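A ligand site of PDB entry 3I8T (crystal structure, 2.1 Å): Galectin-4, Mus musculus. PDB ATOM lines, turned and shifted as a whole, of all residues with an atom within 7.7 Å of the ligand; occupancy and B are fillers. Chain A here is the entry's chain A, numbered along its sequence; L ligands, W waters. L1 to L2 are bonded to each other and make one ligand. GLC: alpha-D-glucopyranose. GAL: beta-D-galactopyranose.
The guanidinium group (NE) of Arg 79 is in hydrogen-bond range of the side-chain amide oxygen (OD1) of Asn 77, 2.7 Å away. OE2 of Glu 99 lies within salt-bridge range of NH2 of Arg 79, at 3.8 Å. O of Asn 89 sits at hydrogen-bond distance from N of His 75 (2.8 Å). The side-chain amide oxygen of Asn 61 is in hydrogen-bond range of a ring nitrogen (ND1) of His 75 (2.5 Å). OD1 of Asn 89 sits close to O of Lys 98, 3.5 Å away. The backbone carbonyl oxygen (O) of Lys 85 lies within hydrogen-bond range of the backbone NH (N) of Arg 79 (2.8 Å). The backbone carbonyl oxygen of Val 87 lies within hydrogen-bond range of the backbone NH of Asn 77. The side-chain amide nitrogen (ND2) of Asn 77 lies within hydrogen-bond range of the backbone carbonyl oxygen (O) of Phe 58 (2.9 Å).
O6 of GAL L2 is in hydrogen-bond range of OE2 of Glu 99, 2.6 Å away. O3 of GLC L1 lies within hydrogen-bond range of NH1 of Arg 79 (2.7 Å). O4 of GAL L2 sits at hydrogen-bond distance from NE2 of His 75. O6 of GAL L2 lies within hydrogen-bond range of ND2 of Asn 89, at 2.9 Å. The side-chain amide oxygen (OD1) of Asn 77 lies within hydrogen-bond range of an oxygen (O4) of GAL L2 (3.0 Å).
Water W3 bridges O2 of GLC L1 (2.7 Å) and OE1 of Glu 99 (2.7 Å). Water W4 lies within hydrogen-bond range of an oxygen (O6) of GLC L1 and the side-chain carboxylate (OE2) of Glu 99. Water W1 lies within hydrogen-bond range of NH2 of Arg 57 and O4 of GLC L1.
Merely in contact with the ligand: Trp 96 (3.7 Å). Hydrophobic or aromatic side chains within 4 Å of the ligand: His 75 and Trp 96. Of the 20 residues printed, 6 come within 4 Å of the ligand. The nearest printed residue that does not touch the ligand is Val 87 (4.1 Å).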
ATOM      1  N   ARG A  57      29.694 -14.993   5.067  1.00  0.00           N
ATOM      2  CA  ARG A  57      29.834 -13.633   5.578  1.00  0.00           C
ATOM      3  C   ARG A  57      29.331 -13.443   7.006  1.00  0.00           C
ATOM      4  O   ARG A  57      28.663 -14.309   7.537  1.00  0.00           O
ATOM      5  CB  ARG A  57      29.203 -12.591   4.625  1.00  0.00           C
ATOM      6  CG  ARG A  57      27.823 -12.863   4.105  1.00  0.00           C
ATOM      7  CD  ARG A  57      27.348 -11.672   3.238  1.00  0.00           C
ATOM      8  NE  ARG A  57      27.532 -11.801   1.783  1.00  0.00           N
ATOM      9  CZ  ARG A  57      26.932 -11.014   0.870  1.00  0.00           C
ATOM     10  NH1 ARG A  57      27.137 -11.221  -0.435  1.00  0.00           N
ATOM     11  NH2 ARG A  57      26.097 -10.049   1.254  1.00  0.00           N
ATOM     12  N   PHE A  58      29.710 -12.331   7.629  1.00  0.00           N
ATOM     13  CA  PHE A  58      29.070 -11.913   8.872  1.00  0.00           C
ATOM     14  C   PHE A  58      29.122 -10.405   8.943  1.00  0.00           C
ATOM     15  O   PHE A  58      29.801  -9.758   8.121  1.00  0.00           O
ATOM     16  CB  PHE A  58      29.657 -12.632  10.134  1.00  0.00           C
ATOM     17  CG  PHE A  58      31.091 -12.215  10.553  1.00  0.00           C
ATOM     18  CD1 PHE A  58      32.165 -13.052  10.274  1.00  0.00           C
ATOM     19  CD2 PHE A  58      31.307 -11.058  11.318  1.00  0.00           C
ATOM     20  CE1 PHE A  58      33.474 -12.718  10.668  1.00  0.00           C
ATOM     21  CE2 PHE A  58      32.630 -10.688  11.737  1.00  0.00           C
ATOM     22  CZ  PHE A  58      33.706 -11.542  11.417  1.00  0.00           C
ATOM     23  N   HIS A  59      28.427  -9.831   9.915  1.00  0.00           N
ATOM     24  CA  HIS A  59      28.561  -8.401  10.086  1.00  0.00           C
ATOM     25  C   HIS A  59      28.550  -7.980  11.555  1.00  0.00           C
ATOM     26  O   HIS A  59      28.055  -8.704  12.423  1.00  0.00           O
ATOM     27  CB  HIS A  59      27.436  -7.638   9.316  1.00  0.00           C
ATOM     28  CG  HIS A  59      26.068  -7.912   9.836  1.00  0.00           C
ATOM     29  ND1 HIS A  59      25.280  -8.923   9.339  1.00  0.00           N
ATOM     30  CD2 HIS A  59      25.350  -7.341  10.841  1.00  0.00           C
ATOM     31  CE1 HIS A  59      24.140  -8.965  10.001  1.00  0.00           C
ATOM     32  NE2 HIS A  59      24.152  -8.008  10.917  1.00  0.00           N
ATOM     33  N   ASN A  61      27.154  -4.402  13.346  1.00  0.00           N
ATOM     34  CA  ASN A  61      26.494  -3.127  13.158  1.00  0.00           C
ATOM     35  C   ASN A  61      26.575  -2.280  14.424  1.00  0.00           C
ATOM     36  O   ASN A  61      26.271  -2.742  15.504  1.00  0.00           O
ATOM     37  CB  ASN A  61      25.018  -3.330  12.807  1.00  0.00           C
ATOM     38  CG  ASN A  61      24.825  -3.918  11.442  1.00  0.00           C
ATOM     39  OD1 ASN A  61      25.712  -3.831  10.607  1.00  0.00           O
ATOM     40  ND2 ASN A  61      23.672  -4.553  11.215  1.00  0.00           N
ATOM     41  N   HIS A  75      28.375  -0.370   9.435  1.00  0.00           N
ATOM     42  CA  HIS A  75      28.190  -1.777   9.106  1.00  0.00           C
ATOM     43  C   HIS A  75      29.549  -2.298   8.612  1.00  0.00           C
ATOM     44  O   HIS A  75      30.090  -1.846   7.574  1.00  0.00           O
ATOM     45  CB  HIS A  75      27.129  -1.849   7.970  1.00  0.00           C
ATOM     46  CG  HIS A  75      26.853  -3.234   7.433  1.00  0.00           C
ATOM     47  ND1 HIS A  75      26.181  -4.195   8.149  1.00  0.00           N
ATOM     48  CD2 HIS A  75      27.015  -3.746   6.185  1.00  0.00           C
ATOM     49  CE1 HIS A  75      25.994  -5.268   7.398  1.00  0.00           C
ATOM     50  NE2 HIS A  75      26.515  -5.024   6.207  1.00  0.00           N
ATOM     51  N   PHE A  76      30.049  -3.318   9.307  1.00  0.00           N
ATOM     52  CA  PHE A  76      31.359  -3.906   9.018  1.00  0.00           C
ATOM     53  C   PHE A  76      31.052  -5.354   8.574  1.00  0.00           C
ATOM     54  O   PHE A  76      30.485  -6.128   9.338  1.00  0.00           O
ATOM     55  CB  PHE A  76      32.221  -3.921  10.307  1.00  0.00           C
ATOM     56  CG  PHE A  76      33.520  -4.709  10.189  1.00  0.00           C
ATOM     57  CD1 PHE A  76      34.641  -4.132   9.637  1.00  0.00           C
ATOM     58  CD2 PHE A  76      33.594  -6.052  10.618  1.00  0.00           C
ATOM     59  CE1 PHE A  76      35.851  -4.858   9.484  1.00  0.00           C
ATOM     60  CE2 PHE A  76      34.771  -6.773  10.504  1.00  0.00           C
ATOM     61  CZ  PHE A  76      35.916  -6.199   9.930  1.00  0.00           C
ATOM     62  N   ASN A  77      31.441  -5.726   7.357  1.00  0.00           N
ATOM     63  CA  ASN A  77      30.814  -6.856   6.680  1.00  0.00           C
ATOM     64  C   ASN A  77      31.814  -7.656   5.814  1.00  0.00           C
ATOM     65  O   ASN A  77      31.858  -7.494   4.585  1.00  0.00           O
ATOM     66  CB  ASN A  77      29.584  -6.357   5.870  1.00  0.00           C
ATOM     67  CG  ASN A  77      28.855  -7.481   5.059  1.00  0.00           C
ATOM     68  OD1 ASN A  77      28.397  -7.233   3.937  1.00  0.00           O
ATOM     69  ND2 ASN A  77      28.716  -8.673   5.652  1.00  0.00           N
ATOM     70  N   ARG A  79      33.158 -10.651   3.641  1.00  0.00           N
ATOM     71  CA  ARG A  79      32.472 -11.525   2.680  1.00  0.00           C
ATOM     72  C   ARG A  79      33.496 -12.339   1.947  1.00  0.00           C
ATOM     73  O   ARG A  79      34.355 -11.767   1.301  1.00  0.00           O
ATOM     74  CB  ARG A  79      31.687 -10.718   1.628  1.00  0.00           C
ATOM     75  CG  ARG A  79      30.679  -9.678   2.146  1.00  0.00           C
ATOM     76  CD  ARG A  79      30.000  -8.982   0.966  1.00  0.00           C
ATOM     77  NE  ARG A  79      28.994  -8.025   1.417  1.00  0.00           N
ATOM     78  CZ  ARG A  79      28.193  -7.298   0.631  1.00  0.00           C
ATOM     79  NH1 ARG A  79      28.232  -7.427  -0.692  1.00  0.00           N
ATOM     80  NH2 ARG A  79      27.316  -6.438   1.182  1.00  0.00           N
ATOM     81  N   LYS A  85      36.715 -10.012   0.594  1.00  0.00           N
ATOM     82  CA  LYS A  85      36.787  -8.558   0.834  1.00  0.00           C
ATOM     83  C   LYS A  85      36.024  -8.263   2.113  1.00  0.00           C
ATOM     84  O   LYS A  85      35.299  -9.140   2.631  1.00  0.00           O
ATOM     85  CB  LYS A  85      36.141  -7.755  -0.320  1.00  0.00           C
ATOM     86  CG  LYS A  85      34.633  -8.090  -0.462  1.00  0.00           C
ATOM     87  CD  LYS A  85      33.908  -7.243  -1.470  1.00  0.00           C
ATOM     88  CE  LYS A  85      34.004  -7.780  -2.866  1.00  0.00           C
ATOM     89  NZ  LYS A  85      33.403  -9.135  -3.044  1.00  0.00           N
ATOM     90  N   VAL A  87      33.236  -5.254   3.288  1.00  0.00           N
ATOM     91  CA  VAL A  87      32.383  -4.179   2.849  1.00  0.00           C
ATOM     92  C   VAL A  87      32.061  -3.328   4.078  1.00  0.00           C
ATOM     93  O   VAL A  87      31.922  -3.852   5.182  1.00  0.00           O
ATOM     94  CB  VAL A  87      31.104  -4.727   2.172  1.00  0.00           C
ATOM     95  CG1 VAL A  87      30.006  -3.668   2.120  1.00  0.00           C
ATOM     96  CG2 VAL A  87      31.426  -5.239   0.797  1.00  0.00           C
ATOM     97  N   PHE A  88      32.027  -2.014   3.901  1.00  0.00           N
ATOM     98  CA  PHE A  88      31.715  -1.074   4.982  1.00  0.00           C
ATOM     99  C   PHE A  88      30.632  -0.148   4.466  1.00  0.00           C
ATOM    100  O   PHE A  88      30.712   0.336   3.317  1.00  0.00           O
ATOM    101  CB  PHE A  88      32.942  -0.208   5.349  1.00  0.00           C
ATOM    102  CG  PHE A  88      34.247  -0.968   5.461  1.00  0.00           C
ATOM    103  CD1 PHE A  88      34.635  -1.523   6.684  1.00  0.00           C
ATOM    104  CD2 PHE A  88      35.082  -1.092   4.373  1.00  0.00           C
ATOM    105  CE1 PHE A  88      35.871  -2.203   6.823  1.00  0.00           C
ATOM    106  CE2 PHE A  88      36.305  -1.815   4.500  1.00  0.00           C
ATOM    107  CZ  PHE A  88      36.660  -2.387   5.742  1.00  0.00           C
ATOM    108  N   ASN A  89      29.626   0.116   5.299  1.00  0.00           N
ATOM    109  CA  ASN A  89      28.507   0.985   4.839  1.00  0.00           C
ATOM    110  C   ASN A  89      27.745   1.580   6.031  1.00  0.00           C
ATOM    111  O   ASN A  89      28.076   1.268   7.202  1.00  0.00           O
ATOM    112  CB  ASN A  89      27.554   0.247   3.866  1.00  0.00           C
ATOM    113  CG  ASN A  89      26.952   1.194   2.804  1.00  0.00           C
ATOM    114  OD1 ASN A  89      26.952   2.422   2.970  1.00  0.00           O
ATOM    115  ND2 ASN A  89      26.444   0.624   1.725  1.00  0.00           N
ATOM    116  N   THR A  90      26.770   2.439   5.714  1.00  0.00           N
ATOM    117  CA  THR A  90      25.913   3.112   6.680  1.00  0.00           C
ATOM    118  C   THR A  90      24.520   2.973   6.117  1.00  0.00           C
ATOM    119  O   THR A  90      24.331   3.135   4.905  1.00  0.00           O
ATOM    120  CB  THR A  90      26.315   4.630   6.818  1.00  0.00           C
ATOM    121  OG1 THR A  90      27.587   4.731   7.507  1.00  0.00           O
ATOM    122  CG2 THR A  90      25.254   5.430   7.613  1.00  0.00           C
ATOM    123  N   MET A  91      23.549   2.653   6.972  1.00  0.00           N
ATOM    124  CA  MET A  91      22.148   2.683   6.586  1.00  0.00           C
ATOM    125  C   MET A  91      21.515   3.894   7.275  1.00  0.00           C
ATOM    126  O   MET A  91      21.585   4.029   8.513  1.00  0.00           O
ATOM    127  CB  MET A  91      21.443   1.416   7.045  1.00  0.00           C
ATOM    128  CG  MET A  91      19.917   1.543   6.879  1.00  0.00           C
ATOM    129  SD  MET A  91      19.037  -0.035   6.930  1.00  0.00           S
ATOM    130  CE  MET A  91      19.483  -0.644   5.334  1.00  0.00           C
ATOM    131  N   GLN A  95      18.134   3.401   4.225  1.00  0.00           N
ATOM    132  CA  GLN A  95      18.791   3.170   2.915  1.00  0.00           C
ATOM    133  C   GLN A  95      20.289   3.039   3.091  1.00  0.00           C
ATOM    134  O   GLN A  95      20.886   3.893   3.750  1.00  0.00           O
ATOM    135  CB  GLN A  95      18.513   4.324   1.953  1.00  0.00           C
ATOM    136  CG  GLN A  95      17.071   4.416   1.476  1.00  0.00           C
ATOM    137  CD  GLN A  95      16.823   3.625   0.207  1.00  0.00           C
ATOM    138  OE1 GLN A  95      16.787   4.194  -0.882  1.00  0.00           O
ATOM    139  NE2 GLN A  95      16.651   2.290   0.338  1.00  0.00           N
ATOM    140  N   TRP A  96      20.885   2.001   2.488  1.00  0.00           N
ATOM    141  CA  TRP A  96      22.326   1.822   2.423  1.00  0.00           C
ATOM    142  C   TRP A  96      22.959   2.927   1.587  1.00  0.00           C
ATOM    143  O   TRP A  96      22.438   3.283   0.514  1.00  0.00           O
ATOM    144  CB  TRP A  96      22.688   0.474   1.782  1.00  0.00           C
ATOM    145  CG  TRP A  96      22.377  -0.661   2.677  1.00  0.00           C
ATOM    146  CD1 TRP A  96      21.448  -1.627   2.465  1.00  0.00           C
ATOM    147  CD2 TRP A  96      22.946  -0.928   3.982  1.00  0.00           C
ATOM    148  NE1 TRP A  96      21.418  -2.506   3.524  1.00  0.00           N
ATOM    149  CE2 TRP A  96      22.325  -2.114   4.470  1.00  0.00           C
ATOM    150  CE3 TRP A  96      23.946  -0.314   4.748  1.00  0.00           C
ATOM    151  CZ2 TRP A  96      22.651  -2.684   5.710  1.00  0.00           C
ATOM    152  CZ3 TRP A  96      24.290  -0.872   5.984  1.00  0.00           C
ATOM    153  CH2 TRP A  96      23.621  -2.048   6.460  1.00  0.00           C
ATOM    154  N   GLY A  97      24.089   3.432   2.070  1.00  0.00           N
ATOM    155  CA  GLY A  97      24.813   4.479   1.336  1.00  0.00           C
ATOM    156  C   GLY A  97      25.785   3.873   0.348  1.00  0.00           C
ATOM    157  O   GLY A  97      25.591   2.728  -0.101  1.00  0.00           O
ATOM    158  N   LYS A  98      26.815   4.644   0.021  1.00  0.00           N
ATOM    159  CA  LYS A  98      27.877   4.200  -0.888  1.00  0.00           C
ATOM    160  C   LYS A  98      28.819   3.243  -0.168  1.00  0.00           C
ATOM    161  O   LYS A  98      29.426   3.620   0.822  1.00  0.00           O
ATOM    162  CB  LYS A  98      28.702   5.382  -1.383  1.00  0.00           C
ATOM    163  CG  LYS A  98      27.955   6.375  -2.273  1.00  0.00           C
ATOM    164  CD  LYS A  98      28.751   7.700  -2.290  1.00  0.00           C
ATOM    165  CE  LYS A  98      28.127   8.759  -3.187  1.00  0.00           C
ATOM    166  NZ  LYS A  98      28.794  10.097  -2.866  1.00  0.00           N
ATOM    167  N   GLU A  99      28.918   2.007  -0.641  1.00  0.00           N
ATOM    168  CA  GLU A  99      29.776   1.002   0.002  1.00  0.00           C
ATOM    169  C   GLU A  99      31.198   1.437  -0.169  1.00  0.00           C
ATOM    170  O   GLU A  99      31.567   1.931  -1.234  1.00  0.00           O
ATOM    171  CB  GLU A  99      29.660  -0.379  -0.684  1.00  0.00           C
ATOM    172  CG  GLU A  99      28.353  -1.021  -0.483  1.00  0.00           C
ATOM    173  CD  GLU A  99      28.272  -2.466  -1.015  1.00  0.00           C
ATOM    174  OE1 GLU A  99      29.123  -2.921  -1.819  1.00  0.00           O
ATOM    175  OE2 GLU A  99      27.311  -3.130  -0.602  1.00  0.00           O
ATOM    176  N   GLU A 100      31.970   1.258   0.887  1.00  0.00           N
ATOM    177  CA  GLU A 100      33.403   1.237   0.824  1.00  0.00           C
ATOM    178  C   GLU A 100      33.794  -0.230   0.880  1.00  0.00           C
ATOM    179  O   GLU A 100      33.051  -1.062   1.407  1.00  0.00           O
ATOM    180  CB  GLU A 100      34.005   2.068   1.984  1.00  0.00           C
ATOM    181  CG  GLU A 100      33.792   3.615   1.768  1.00  0.00           C
ATOM    182  CD  GLU A 100      34.139   4.445   3.011  1.00  0.00           C
ATOM    183  OE1 GLU A 100      35.187   4.171   3.651  1.00  0.00           O
ATOM    184  OE2 GLU A 100      33.371   5.367   3.363  1.00  0.00           O
HETATM  185  C1  GLC L   1      24.208  -4.481  -4.406  1.00  0.00           C
HETATM  186  C2  GLC L   1      25.505  -4.624  -3.614  1.00  0.00           C
HETATM  187  C3  GLC L   1      25.312  -5.512  -2.384  1.00  0.00           C
HETATM  188  C4  GLC L   1      24.142  -5.008  -1.574  1.00  0.00           C
HETATM  189  C5  GLC L   1      22.866  -4.858  -2.445  1.00  0.00           C
HETATM  190  C6  GLC L   1      21.684  -4.208  -1.710  1.00  0.00           C
HETATM  191  O1  GLC L   1      23.895  -5.726  -5.018  1.00  0.00           O
HETATM  192  O2  GLC L   1      26.472  -5.185  -4.465  1.00  0.00           O
HETATM  193  O3  GLC L   1      26.507  -5.515  -1.642  1.00  0.00           O
HETATM  194  O4  GLC L   1      23.950  -5.886  -0.499  1.00  0.00           O
HETATM  195  O5  GLC L   1      23.145  -4.049  -3.583  1.00  0.00           O
HETATM  196  O6  GLC L   1      21.973  -2.849  -1.340  1.00  0.00           O
HETATM  197  C1  GAL L   2      23.736  -5.346   0.779  1.00  0.00           C
HETATM  198  C2  GAL L   2      23.358  -6.471   1.753  1.00  0.00           C
HETATM  199  C3  GAL L   2      23.296  -5.872   3.168  1.00  0.00           C
HETATM  200  C4  GAL L   2      24.553  -5.083   3.491  1.00  0.00           C
HETATM  201  C5  GAL L   2      24.780  -4.008   2.433  1.00  0.00           C
HETATM  202  C6  GAL L   2      25.984  -3.066   2.737  1.00  0.00           C
HETATM  203  O2  GAL L   2      22.094  -7.033   1.403  1.00  0.00           O
HETATM  204  O3  GAL L   2      23.123  -6.879   4.133  1.00  0.00           O
HETATM  205  O4  GAL L   2      25.692  -5.919   3.516  1.00  0.00           O
HETATM  206  O5  GAL L   2      24.948  -4.682   1.204  1.00  0.00           O
HETATM  207  O6  GAL L   2      26.223  -2.261   1.603  1.00  0.00           O
HETATM  208  O   HOH W   1      24.667  -8.711  -0.868  1.00  0.00           O
HETATM  209  O   HOH W   2      23.247  -7.284   6.817  1.00  0.00           O
HETATM  210  O   HOH W   3      29.019  -4.935  -3.642  1.00  0.00           O
HETATM  211  O   HOH W   4      24.339  -1.491  -0.650  1.00  0.00           O
